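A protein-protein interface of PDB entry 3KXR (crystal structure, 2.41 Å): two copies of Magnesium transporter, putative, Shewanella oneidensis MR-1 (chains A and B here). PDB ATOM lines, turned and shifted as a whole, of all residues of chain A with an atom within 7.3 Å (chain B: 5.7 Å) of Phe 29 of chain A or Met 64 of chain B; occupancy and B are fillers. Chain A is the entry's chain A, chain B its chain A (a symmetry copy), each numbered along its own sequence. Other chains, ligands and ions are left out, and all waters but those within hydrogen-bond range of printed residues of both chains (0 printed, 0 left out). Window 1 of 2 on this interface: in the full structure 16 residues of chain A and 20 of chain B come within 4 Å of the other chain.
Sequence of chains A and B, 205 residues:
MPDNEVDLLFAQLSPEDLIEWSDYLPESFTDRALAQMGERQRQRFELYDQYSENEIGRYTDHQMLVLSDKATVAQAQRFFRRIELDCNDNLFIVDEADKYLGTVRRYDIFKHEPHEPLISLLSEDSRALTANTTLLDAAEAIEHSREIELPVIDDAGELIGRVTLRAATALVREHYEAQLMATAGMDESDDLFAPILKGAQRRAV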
ATOM      1  N   LEU A   9      15.978 -14.269   6.774  1.00  0.00           N
ATOM      2  CA  LEU A   9      17.032 -15.300   6.730  1.00  0.00           C
ATOM      3  C   LEU A   9      16.657 -16.552   5.949  1.00  0.00           C
ATOM      4  O   LEU A   9      17.381 -17.001   5.051  1.00  0.00           O
ATOM      5  CB  LEU A   9      17.406 -15.747   8.156  1.00  0.00           C
ATOM      6  CG  LEU A   9      18.451 -16.872   8.302  1.00  0.00           C
ATOM      7  CD1 LEU A   9      19.742 -16.454   7.649  1.00  0.00           C
ATOM      8  CD2 LEU A   9      18.708 -17.293   9.755  1.00  0.00           C
ATOM      9  N   PHE A  10      15.542 -17.147   6.336  1.00  0.00           N
ATOM     10  CA  PHE A  10      15.131 -18.392   5.726  1.00  0.00           C
ATOM     11  C   PHE A  10      14.693 -18.112   4.282  1.00  0.00           C
ATOM     12  O   PHE A  10      14.826 -18.978   3.427  1.00  0.00           O
ATOM     13  CB  PHE A  10      14.078 -19.104   6.593  1.00  0.00           C
ATOM     14  CG  PHE A  10      14.531 -19.325   8.054  1.00  0.00           C
ATOM     15  CD1 PHE A  10      15.398 -20.385   8.395  1.00  0.00           C
ATOM     16  CD2 PHE A  10      14.111 -18.453   9.089  1.00  0.00           C
ATOM     17  CE1 PHE A  10      15.827 -20.594   9.750  1.00  0.00           C
ATOM     18  CE2 PHE A  10      14.542 -18.643  10.453  1.00  0.00           C
ATOM     19  CZ  PHE A  10      15.396 -19.713  10.775  1.00  0.00           C
ATOM     20  N   LEU A  13      17.910 -18.736   2.045  1.00  0.00           N
ATOM     21  CA  LEU A  13      18.479 -20.084   1.894  1.00  0.00           C
ATOM     22  C   LEU A  13      17.590 -20.979   1.054  1.00  0.00           C
ATOM     23  O   LEU A  13      16.434 -21.130   1.355  1.00  0.00           O
ATOM     24  CB  LEU A  13      18.631 -20.748   3.259  1.00  0.00           C
ATOM     25  CG  LEU A  13      19.884 -20.435   4.073  1.00  0.00           C
ATOM     26  CD1 LEU A  13      19.879 -21.330   5.272  1.00  0.00           C
ATOM     27  CD2 LEU A  13      21.194 -20.641   3.295  1.00  0.00           C
ATOM     28  N   LEU A  18      20.093 -26.241   2.128  1.00  0.00           N
ATOM     29  CA  LEU A  18      19.849 -27.019   3.331  1.00  0.00           C
ATOM     30  C   LEU A  18      20.383 -28.427   3.168  1.00  0.00           C
ATOM     31  O   LEU A  18      21.073 -28.918   4.046  1.00  0.00           O
ATOM     32  CB  LEU A  18      18.364 -27.039   3.698  1.00  0.00           C
ATOM     33  CG  LEU A  18      17.743 -25.708   4.152  1.00  0.00           C
ATOM     34  CD1 LEU A  18      16.229 -25.861   4.366  1.00  0.00           C
ATOM     35  CD2 LEU A  18      18.414 -25.166   5.441  1.00  0.00           C
ATOM     36  N   TRP A  21      24.081 -28.664   3.168  1.00  0.00           N
ATOM     37  CA  TRP A  21      24.592 -28.437   4.516  1.00  0.00           C
ATOM     38  C   TRP A  21      23.961 -29.290   5.609  1.00  0.00           C
ATOM     39  O   TRP A  21      23.967 -28.915   6.796  1.00  0.00           O
ATOM     40  CB  TRP A  21      24.444 -26.965   4.837  1.00  0.00           C
ATOM     41  CG  TRP A  21      25.673 -26.249   4.552  1.00  0.00           C
ATOM     42  CD1 TRP A  21      26.728 -26.686   3.801  1.00  0.00           C
ATOM     43  CD2 TRP A  21      26.015 -24.962   5.013  1.00  0.00           C
ATOM     44  NE1 TRP A  21      27.708 -25.752   3.784  1.00  0.00           N
ATOM     45  CE2 TRP A  21      27.299 -24.676   4.526  1.00  0.00           C
ATOM     46  CE3 TRP A  21      25.367 -24.021   5.811  1.00  0.00           C
ATOM     47  CZ2 TRP A  21      27.953 -23.476   4.802  1.00  0.00           C
ATOM     48  CZ3 TRP A  21      26.019 -22.819   6.093  1.00  0.00           C
ATOM     49  CH2 TRP A  21      27.292 -22.555   5.588  1.00  0.00           C
ATOM     50  N   LEU A  25      24.084 -28.252   9.780  1.00  0.00           N
ATOM     51  CA  LEU A  25      22.973 -27.519  10.396  1.00  0.00           C
ATOM     52  C   LEU A  25      22.262 -28.452  11.354  1.00  0.00           C
ATOM     53  O   LEU A  25      22.009 -29.587  10.989  1.00  0.00           O
ATOM     54  CB  LEU A  25      21.975 -27.083   9.327  1.00  0.00           C
ATOM     55  CG  LEU A  25      22.478 -26.031   8.338  1.00  0.00           C
ATOM     56  CD1 LEU A  25      21.525 -25.889   7.142  1.00  0.00           C
ATOM     57  CD2 LEU A  25      22.696 -24.682   9.035  1.00  0.00           C
ATOM     58  N   PRO A  26      21.907 -27.970  12.562  1.00  0.00           N
ATOM     59  CA  PRO A  26      21.007 -28.687  13.474  1.00  0.00           C
ATOM     60  C   PRO A  26      19.659 -28.975  12.817  1.00  0.00           C
ATOM     61  O   PRO A  26      19.177 -28.168  11.988  1.00  0.00           O
ATOM     62  CB  PRO A  26      20.782 -27.703  14.604  1.00  0.00           C
ATOM     63  CG  PRO A  26      21.764 -26.615  14.408  1.00  0.00           C
ATOM     64  CD  PRO A  26      22.172 -26.595  13.007  1.00  0.00           C
ATOM     65  N   GLU A  27      19.053 -30.108  13.164  1.00  0.00           N
ATOM     66  CA  GLU A  27      17.789 -30.481  12.553  1.00  0.00           C
ATOM     67  C   GLU A  27      16.767 -29.391  12.882  1.00  0.00           C
ATOM     68  O   GLU A  27      15.949 -29.047  12.027  1.00  0.00           O
ATOM     69  CB  GLU A  27      17.334 -31.900  12.969  1.00  0.00           C
ATOM     70  CG  GLU A  27      17.885 -33.063  12.048  1.00  0.00           C
ATOM     71  N   SER A  28      16.870 -28.807  14.079  1.00  0.00           N
ATOM     72  CA  SER A  28      15.969 -27.741  14.529  1.00  0.00           C
ATOM     73  C   SER A  28      15.977 -26.568  13.549  1.00  0.00           C
ATOM     74  O   SER A  28      14.931 -25.981  13.228  1.00  0.00           O
ATOM     75  CB  SER A  28      16.318 -27.265  15.954  1.00  0.00           C
ATOM     76  OG  SER A  28      17.545 -26.538  16.041  1.00  0.00           O
ATOM     77  N   PHE A  29      17.152 -26.251  13.044  1.00  0.00           N
ATOM     78  CA  PHE A  29      17.308 -25.146  12.121  1.00  0.00           C
ATOM     79  C   PHE A  29      16.693 -25.530  10.767  1.00  0.00           C
ATOM     80  O   PHE A  29      15.992 -24.734  10.137  1.00  0.00           O
ATOM     81  CB  PHE A  29      18.800 -24.814  11.988  1.00  0.00           C
ATOM     82  CG  PHE A  29      19.090 -23.742  11.008  1.00  0.00           C
ATOM     83  CD1 PHE A  29      19.355 -22.455  11.422  1.00  0.00           C
ATOM     84  CD2 PHE A  29      19.103 -24.017   9.657  1.00  0.00           C
ATOM     85  CE1 PHE A  29      19.613 -21.440  10.509  1.00  0.00           C
ATOM     86  CE2 PHE A  29      19.354 -22.990   8.720  1.00  0.00           C
ATOM     87  CZ  PHE A  29      19.612 -21.704   9.157  1.00  0.00           C
ATOM     88  N   THR A  30      16.953 -26.751  10.327  1.00  0.00           N
ATOM     89  CA  THR A  30      16.403 -27.193   9.076  1.00  0.00           C
ATOM     90  C   THR A  30      14.883 -27.146   9.132  1.00  0.00           C
ATOM     91  O   THR A  30      14.250 -26.581   8.237  1.00  0.00           O
ATOM     92  CB  THR A  30      16.894 -28.590   8.707  1.00  0.00           C
ATOM     93  OG1 THR A  30      18.304 -28.526   8.444  1.00  0.00           O
ATOM     94  CG2 THR A  30      16.154 -29.105   7.451  1.00  0.00           C
ATOM     95  N   ASP A  31      14.310 -27.667  10.212  1.00  0.00           N
ATOM     96  CA  ASP A  31      12.857 -27.662  10.379  1.00  0.00           C
ATOM     97  C   ASP A  31      12.243 -26.276  10.398  1.00  0.00           C
ATOM     98  O   ASP A  31      11.149 -26.095   9.864  1.00  0.00           O
ATOM     99  CB  ASP A  31      12.450 -28.408  11.652  1.00  0.00           C
ATOM    100  CG  ASP A  31      12.813 -29.886  11.594  1.00  0.00           C
ATOM    101  OD1 ASP A  31      13.052 -30.406  10.492  1.00  0.00           O
ATOM    102  OD2 ASP A  31      12.897 -30.528  12.653  1.00  0.00           O
ATOM    103  N   ARG A  32      12.903 -25.304  11.017  1.00  0.00           N
ATOM    104  CA  ARG A  32      12.325 -23.963  11.037  1.00  0.00           C
ATOM    105  C   ARG A  32      12.391 -23.382   9.622  1.00  0.00           C
ATOM    106  O   ARG A  32      11.463 -22.715   9.173  1.00  0.00           O
ATOM    107  CB  ARG A  32      13.024 -23.044  12.050  1.00  0.00           C
ATOM    108  CG  ARG A  32      12.654 -23.353  13.529  1.00  0.00           C
ATOM    109  CD  ARG A  32      13.187 -22.286  14.548  1.00  0.00           C
ATOM    110  NE  ARG A  32      14.515 -21.815  14.121  1.00  0.00           N
ATOM    111  CZ  ARG A  32      15.695 -22.286  14.558  1.00  0.00           C
ATOM    112  NH1 ARG A  32      15.747 -23.263  15.470  1.00  0.00           N
ATOM    113  NH2 ARG A  32      16.837 -21.773  14.079  1.00  0.00           N
ATOM    114  N   ALA A  33      13.487 -23.673   8.918  1.00  0.00           N
ATOM    115  CA  ALA A  33      13.649 -23.246   7.511  1.00  0.00           C
ATOM    116  C   ALA A  33      12.547 -23.816   6.591  1.00  0.00           C
ATOM    117  O   ALA A  33      11.952 -23.089   5.776  1.00  0.00           O
ATOM    118  CB  ALA A  33      15.017 -23.649   6.995  1.00  0.00           C
ATOM    119  N   LEU A  34      12.270 -25.108   6.768  1.00  0.00           N
ATOM    120  CA  LEU A  34      11.271 -25.794   5.986  1.00  0.00           C
ATOM    121  C   LEU A  34       9.871 -25.233   6.255  1.00  0.00           C
ATOM    122  O   LEU A  34       9.099 -25.028   5.320  1.00  0.00           O
ATOM    123  CB  LEU A  34      11.305 -27.301   6.260  1.00  0.00           C
ATOM    124  CG  LEU A  34      12.485 -28.075   5.671  1.00  0.00           C
ATOM    125  CD1 LEU A  34      12.368 -29.531   6.130  1.00  0.00           C
ATOM    126  CD2 LEU A  34      12.563 -27.954   4.134  1.00  0.00           C
ATOM    127  N   ALA A  35       9.561 -24.993   7.525  1.00  0.00           N
ATOM    128  CA  ALA A  35       8.281 -24.413   7.923  1.00  0.00           C
ATOM    129  C   ALA A  35       8.074 -23.021   7.348  1.00  0.00           C
ATOM    130  O   ALA A  35       6.950 -22.607   7.106  1.00  0.00           O
ATOM    131  CB  ALA A  35       8.174 -24.372   9.410  1.00  0.00           C
ATOM    132  N   ASP B  61      14.705 -14.148  19.053  1.00  0.00           N
ATOM    133  CA  ASP B  61      14.610 -14.261  17.620  1.00  0.00           C
ATOM    134  C   ASP B  61      15.245 -15.576  17.220  1.00  0.00           C
ATOM    135  O   ASP B  61      16.355 -15.853  17.586  1.00  0.00           O
ATOM    136  CB  ASP B  61      15.350 -13.079  17.010  1.00  0.00           C
ATOM    137  CG  ASP B  61      15.271 -13.048  15.522  1.00  0.00           C
ATOM    138  OD1 ASP B  61      14.638 -13.941  14.928  1.00  0.00           O
ATOM    139  OD2 ASP B  61      15.872 -12.120  14.951  1.00  0.00           O
ATOM    140  N   HIS B  62      14.520 -16.401  16.486  1.00  0.00           N
ATOM    141  CA  HIS B  62      15.011 -17.712  16.088  1.00  0.00           C
ATOM    142  C   HIS B  62      16.025 -17.600  14.957  1.00  0.00           C
ATOM    143  O   HIS B  62      16.780 -18.536  14.729  1.00  0.00           O
ATOM    144  CB  HIS B  62      13.878 -18.631  15.633  1.00  0.00           C
ATOM    145  CG  HIS B  62      12.939 -19.065  16.730  1.00  0.00           C
ATOM    146  ND1 HIS B  62      13.348 -19.793  17.835  1.00  0.00           N
ATOM    147  CD2 HIS B  62      11.595 -18.898  16.871  1.00  0.00           C
ATOM    148  CE1 HIS B  62      12.302 -20.045  18.607  1.00  0.00           C
ATOM    149  NE2 HIS B  62      11.228 -19.507  18.048  1.00  0.00           N
ATOM    150  N   GLN B  63      16.006 -16.470  14.250  1.00  0.00           N
ATOM    151  CA  GLN B  63      16.950 -16.162  13.154  1.00  0.00           C
ATOM    152  C   GLN B  63      18.365 -15.969  13.637  1.00  0.00           C
ATOM    153  O   GLN B  63      18.662 -15.025  14.354  1.00  0.00           O
ATOM    154  CB  GLN B  63      16.536 -14.871  12.424  1.00  0.00           C
ATOM    155  CG  GLN B  63      15.809 -15.150  11.172  1.00  0.00           C
ATOM    156  CD  GLN B  63      15.041 -13.986  10.619  1.00  0.00           C
ATOM    157  OE1 GLN B  63      15.477 -13.352   9.654  1.00  0.00           O
ATOM    158  NE2 GLN B  63      13.853 -13.742  11.172  1.00  0.00           N
ATOM    159  N   MET B  64      19.253 -16.843  13.223  1.00  0.00           N
ATOM    160  CA  MET B  64      20.602 -16.763  13.694  1.00  0.00           C
ATOM    161  C   MET B  64      21.533 -17.618  12.877  1.00  0.00           C
ATOM    162  O   MET B  64      21.134 -18.514  12.178  1.00  0.00           O
ATOM    163  CB  MET B  64      20.650 -17.228  15.147  1.00  0.00           C
ATOM    164  CG  MET B  64      20.194 -18.656  15.311  1.00  0.00           C
ATOM    165  SD  MET B  64      20.233 -19.271  17.164  1.00  0.00           S
ATOM    166  CE  MET B  64      19.021 -20.854  17.025  1.00  0.00           C
ATOM    167  N   LEU B  65      22.812 -17.337  12.998  1.00  0.00           N
ATOM    168  CA  LEU B  65      23.835 -18.202  12.451  1.00  0.00           C
ATOM    169  C   LEU B  65      24.188 -19.299  13.502  1.00  0.00           C
ATOM    170  O   LEU B  65      24.725 -19.024  14.562  1.00  0.00           O
ATOM    171  CB  LEU B  65      25.034 -17.337  12.020  1.00  0.00           C
ATOM    172  CG  LEU B  65      25.106 -16.861  10.547  1.00  0.00           C
ATOM    173  CD1 LEU B  65      23.814 -16.379   9.955  1.00  0.00           C
ATOM    174  CD2 LEU B  65      26.218 -15.834  10.388  1.00  0.00           C
ATOM    175  N   VAL B  66      23.834 -20.545  13.203  1.00  0.00           N
ATOM    176  CA  VAL B  66      24.163 -21.674  14.066  1.00  0.00           C
ATOM    177  C   VAL B  66      24.685 -22.870  13.220  1.00  0.00           C
ATOM    178  O   VAL B  66      24.212 -23.114  12.116  1.00  0.00           O
ATOM    179  CB  VAL B  66      22.926 -22.084  14.920  1.00  0.00           C
ATOM    180  CG1 VAL B  66      21.705 -22.226  14.024  1.00  0.00           C
ATOM    181  CG2 VAL B  66      23.200 -23.350  15.692  1.00  0.00           C
ATOM    182  N   PHE B  79      28.996 -19.037   5.737  1.00  0.00           N
ATOM    183  CA  PHE B  79      27.743 -18.584   6.342  1.00  0.00           C
ATOM    184  C   PHE B  79      27.723 -17.060   6.468  1.00  0.00           C
ATOM    185  O   PHE B  79      26.721 -16.394   6.194  1.00  0.00           O
ATOM    186  CB  PHE B  79      27.580 -19.213   7.740  1.00  0.00           C
ATOM    187  CG  PHE B  79      26.170 -19.663   8.068  1.00  0.00           C
ATOM    188  CD1 PHE B  79      25.064 -19.098   7.456  1.00  0.00           C
ATOM    189  CD2 PHE B  79      25.965 -20.629   9.047  1.00  0.00           C
ATOM    190  CE1 PHE B  79      23.782 -19.512   7.796  1.00  0.00           C
ATOM    191  CE2 PHE B  79      24.688 -21.051   9.407  1.00  0.00           C
ATOM    192  CZ  PHE B  79      23.594 -20.505   8.791  1.00  0.00           C
ATOM    193  N   LEU B  85      22.293 -10.491   7.796  1.00  0.00           N
ATOM    194  CA  LEU B  85      21.457 -10.550   8.968  1.00  0.00           C
ATOM    195  C   LEU B  85      21.747  -9.364   9.874  1.00  0.00           C
ATOM    196  O   LEU B  85      22.904  -8.975  10.060  1.00  0.00           O
ATOM    197  CB  LEU B  85      21.782 -11.813   9.701  1.00  0.00           C
ATOM    198  CG  LEU B  85      20.684 -12.417  10.513  1.00  0.00           C
ATOM    199  CD1 LEU B  85      19.633 -12.870   9.537  1.00  0.00           C
ATOM    200  CD2 LEU B  85      21.306 -13.589  11.291  1.00  0.00           C
ATOM    201  N   PHE B  92      26.865 -19.476  16.391  1.00  0.00           N
ATOM    202  CA  PHE B  92      26.706 -20.303  17.566  1.00  0.00           C
ATOM    203  C   PHE B  92      26.870 -21.767  17.233  1.00  0.00           C
ATOM    204  O   PHE B  92      26.394 -22.212  16.195  1.00  0.00           O
ATOM    205  CB  PHE B  92      25.337 -20.023  18.187  1.00  0.00           C
ATOM    206  CG  PHE B  92      25.127 -18.578  18.462  1.00  0.00           C
ATOM    207  CD1 PHE B  92      26.081 -17.850  19.163  1.00  0.00           C
ATOM    208  CD2 PHE B  92      24.019 -17.908  17.973  1.00  0.00           C
ATOM    209  CE1 PHE B  92      25.906 -16.489  19.394  1.00  0.00           C
ATOM    210  CE2 PHE B  92      23.841 -16.532  18.209  1.00  0.00           C
ATOM    211  CZ  PHE B  92      24.793 -15.833  18.913  1.00  0.00           C
ATOM    212  N   ASP B  98      21.387 -30.222  20.348  1.00  0.00           N
ATOM    213  CA  ASP B  98      21.061 -28.781  20.271  1.00  0.00           C
ATOM    214  C   ASP B  98      21.491 -27.995  21.502  1.00  0.00           C
ATOM    215  O   ASP B  98      21.027 -26.881  21.702  1.00  0.00           O
ATOM    216  CB  ASP B  98      19.543 -28.548  20.045  1.00  0.00           C
ATOM    217  CG  ASP B  98      19.203 -28.054  18.645  1.00  0.00           C
ATOM    218  OD1 ASP B  98      19.633 -26.940  18.237  1.00  0.00           O
ATOM    219  OD2 ASP B  98      18.446 -28.777  17.943  1.00  0.00           O
ATOM    220  N   GLU B 149      24.982  -9.131  19.687  1.00  0.00           N
ATOM    221  CA  GLU B 149      23.916 -10.097  19.842  1.00  0.00           C
ATOM    222  C   GLU B 149      24.349 -11.064  20.894  1.00  0.00           C
ATOM    223  O   GLU B 149      25.547 -11.298  21.069  1.00  0.00           O
ATOM    224  CB  GLU B 149      23.703 -10.855  18.529  1.00  0.00           C
ATOM    225  CG  GLU B 149      24.948 -11.641  18.082  1.00  0.00           C
ATOM    226  CD  GLU B 149      24.871 -12.242  16.673  1.00  0.00           C
ATOM    227  OE1 GLU B 149      23.846 -12.880  16.324  1.00  0.00           O
ATOM    228  OE2 GLU B 149      25.876 -12.108  15.936  1.00  0.00           O
ATOM    229  N   LEU B 159      19.968 -24.092  22.676  1.00  0.00           N
ATOM    230  CA  LEU B 159      19.998 -22.797  22.027  1.00  0.00           C
ATOM    231  C   LEU B 159      18.661 -22.585  21.367  1.00  0.00           C
ATOM    232  O   LEU B 159      18.348 -23.273  20.431  1.00  0.00           O
ATOM    233  CB  LEU B 159      21.099 -22.795  20.955  1.00  0.00           C
ATOM    234  CG  LEU B 159      21.251 -21.518  20.167  1.00  0.00           C
ATOM    235  CD1 LEU B 159      21.475 -20.378  21.168  1.00  0.00           C
ATOM    236  CD2 LEU B 159      22.396 -21.684  19.165  1.00  0.00           C
ATOM    237  N   ILE B 160      17.859 -21.651  21.851  1.00  0.00           N
ATOM    238  CA  ILE B 160      16.570 -21.411  21.212  1.00  0.00           C
ATOM    239  C   ILE B 160      16.537 -20.196  20.282  1.00  0.00           C
ATOM    240  O   ILE B 160      15.592 -20.043  19.501  1.00  0.00           O
ATOM    241  CB  ILE B 160      15.449 -21.311  22.228  1.00  0.00           C
ATOM    242  CG1 ILE B 160      15.607 -20.045  23.060  1.00  0.00           C
ATOM    243  CG2 ILE B 160      15.420 -22.585  23.103  1.00  0.00           C
ATOM    244  CD1 ILE B 160      14.608 -19.980  24.222  1.00  0.00           C
ATOM    245  N   GLY B 161      17.549 -19.340  20.336  1.00  0.00           N
ATOM    246  CA  GLY B 161      17.563 -18.136  19.489  1.00  0.00           C
ATOM    247  C   GLY B 161      18.528 -17.077  19.991  1.00  0.00           C
ATOM    248  O   GLY B 161      19.414 -17.365  20.782  1.00  0.00           O
ATOM    249  N   ARG B 162      18.352 -15.842  19.545  1.00  0.00           N
ATOM    250  CA  ARG B 162      19.249 -14.774  19.974  1.00  0.00           C
ATOM    251  C   ARG B 162      18.481 -13.497  20.262  1.00  0.00           C
ATOM    252  O   ARG B 162      17.344 -13.350  19.832  1.00  0.00           O
ATOM    253  CB  ARG B 162      20.267 -14.501  18.881  1.00  0.00           C
ATOM    254  CG  ARG B 162      19.697 -13.715  17.741  1.00  0.00           C
ATOM    255  CD  ARG B 162      20.627 -13.662  16.566  1.00  0.00           C
ATOM    256  NE  ARG B 162      20.016 -12.893  15.496  1.00  0.00           N
ATOM    257  CZ  ARG B 162      20.545 -11.848  14.854  1.00  0.00           C
ATOM    258  NH1 ARG B 162      21.756 -11.367  15.123  1.00  0.00           N
ATOM    259  NH2 ARG B 162      19.833 -11.260  13.916  1.00  0.00           N
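Phe 29 of chain A touches just these residues of chain B: Met 64 (3.7 Å) and Val 66 (3.5 Å).
Of the printed residues of chain A, Met 64 of chain B touches Leu 9, Phe 29 and Arg 32.
Of the printed residues of chain A, Leu 85 of chain B touches Leu 9.
Of the printed residues of chain B, Trp 21 of chain A touches Phe 79 (3.7 Å).
Leu 13 of chain A touches none of the printed residues of chain B.
Glu 149 of chain B touches none of the printed residues of chain A.
The nearest printed residue of chain A that does not touch Phe 79 of chain B is Leu 25 of chain A (4.2 Å).
N of Leu 9 of chain A is in hydrogen-bond range of OE1 of Gln 63 of chain B (3.1 Å).
The side-chain carboxylate (OD1) of Asp 98 of chain B is in hydrogen-bond range of the side-chain hydroxyl (OG) of Ser 28 of chain A (3.1 Å).
The guanidinium group of Arg 32 of chain A lies within hydrogen-bond range of the backbone carbonyl oxygen of His 62 of chain B (3.3 Å).
Leu 9 of chain A touches Met 64 of chain B.
Leu 9 of chain A touches Leu 85 of chain B.
Phe 10 of chain A touches Gln 63 of chain B (CE2 to CG, 3.8 Å).
CZ3 of Trp 21 of chain A touches CD2 of Phe 79 of chain B, at 3.7 Å.
Val 66 of chain B touches Leu 25 of chain A (O to CD2, 3.8 Å).
CG of Pro 26 of chain A touches CG2 of Val 66 of chain B, 3.8 Å away.
Pro 26 of chain A touches Asp 98 of chain B.
Met 64 of chain B touches Phe 29 of chain A (O to CE1, 3.7 Å).
Phe 29 of chain A touches Val 66 of chain B.
CE of Met 64 of chain B touches NH2 of Arg 32 of chain A, 3.8 Å away.
No position is printed for both chains.
The side-chain carboxylate (OD1) of Asp 61 of chain B sits at hydrogen-bond distance from the backbone NH (N) of Gln 63 of chain B (3.0 Å).
ND1 of His 62 of chain B sits at hydrogen-bond distance from O of Ile 160 of chain B.
The guanidinium group (NE) of Arg 162 of chain B sits at hydrogen-bond distance from the backbone carbonyl oxygen (O) of Gln 63 of chain B, 2.8 Å away.
O of Asp 98 of chain B sits at hydrogen-bond distance from N of Leu 159 of chain B (3.1 Å).
Of the 16 printed residues of chain A, 8 touch a printed residue of chain B.
Hydrophobic or aromatic side chains of chain A within 4 Å of the printed part of chain B: Leu 9, Phe 10, Trp 21, Leu 25, Pro 26 and Phe 29.
Along chain B the printed residues that touch a printed residue of chain A span positions 62 to 98.
Among the printed residues, no Asp or Glu carboxylate lies within 4 Å of a Lys or Arg side-chain nitrogen of the other chain.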
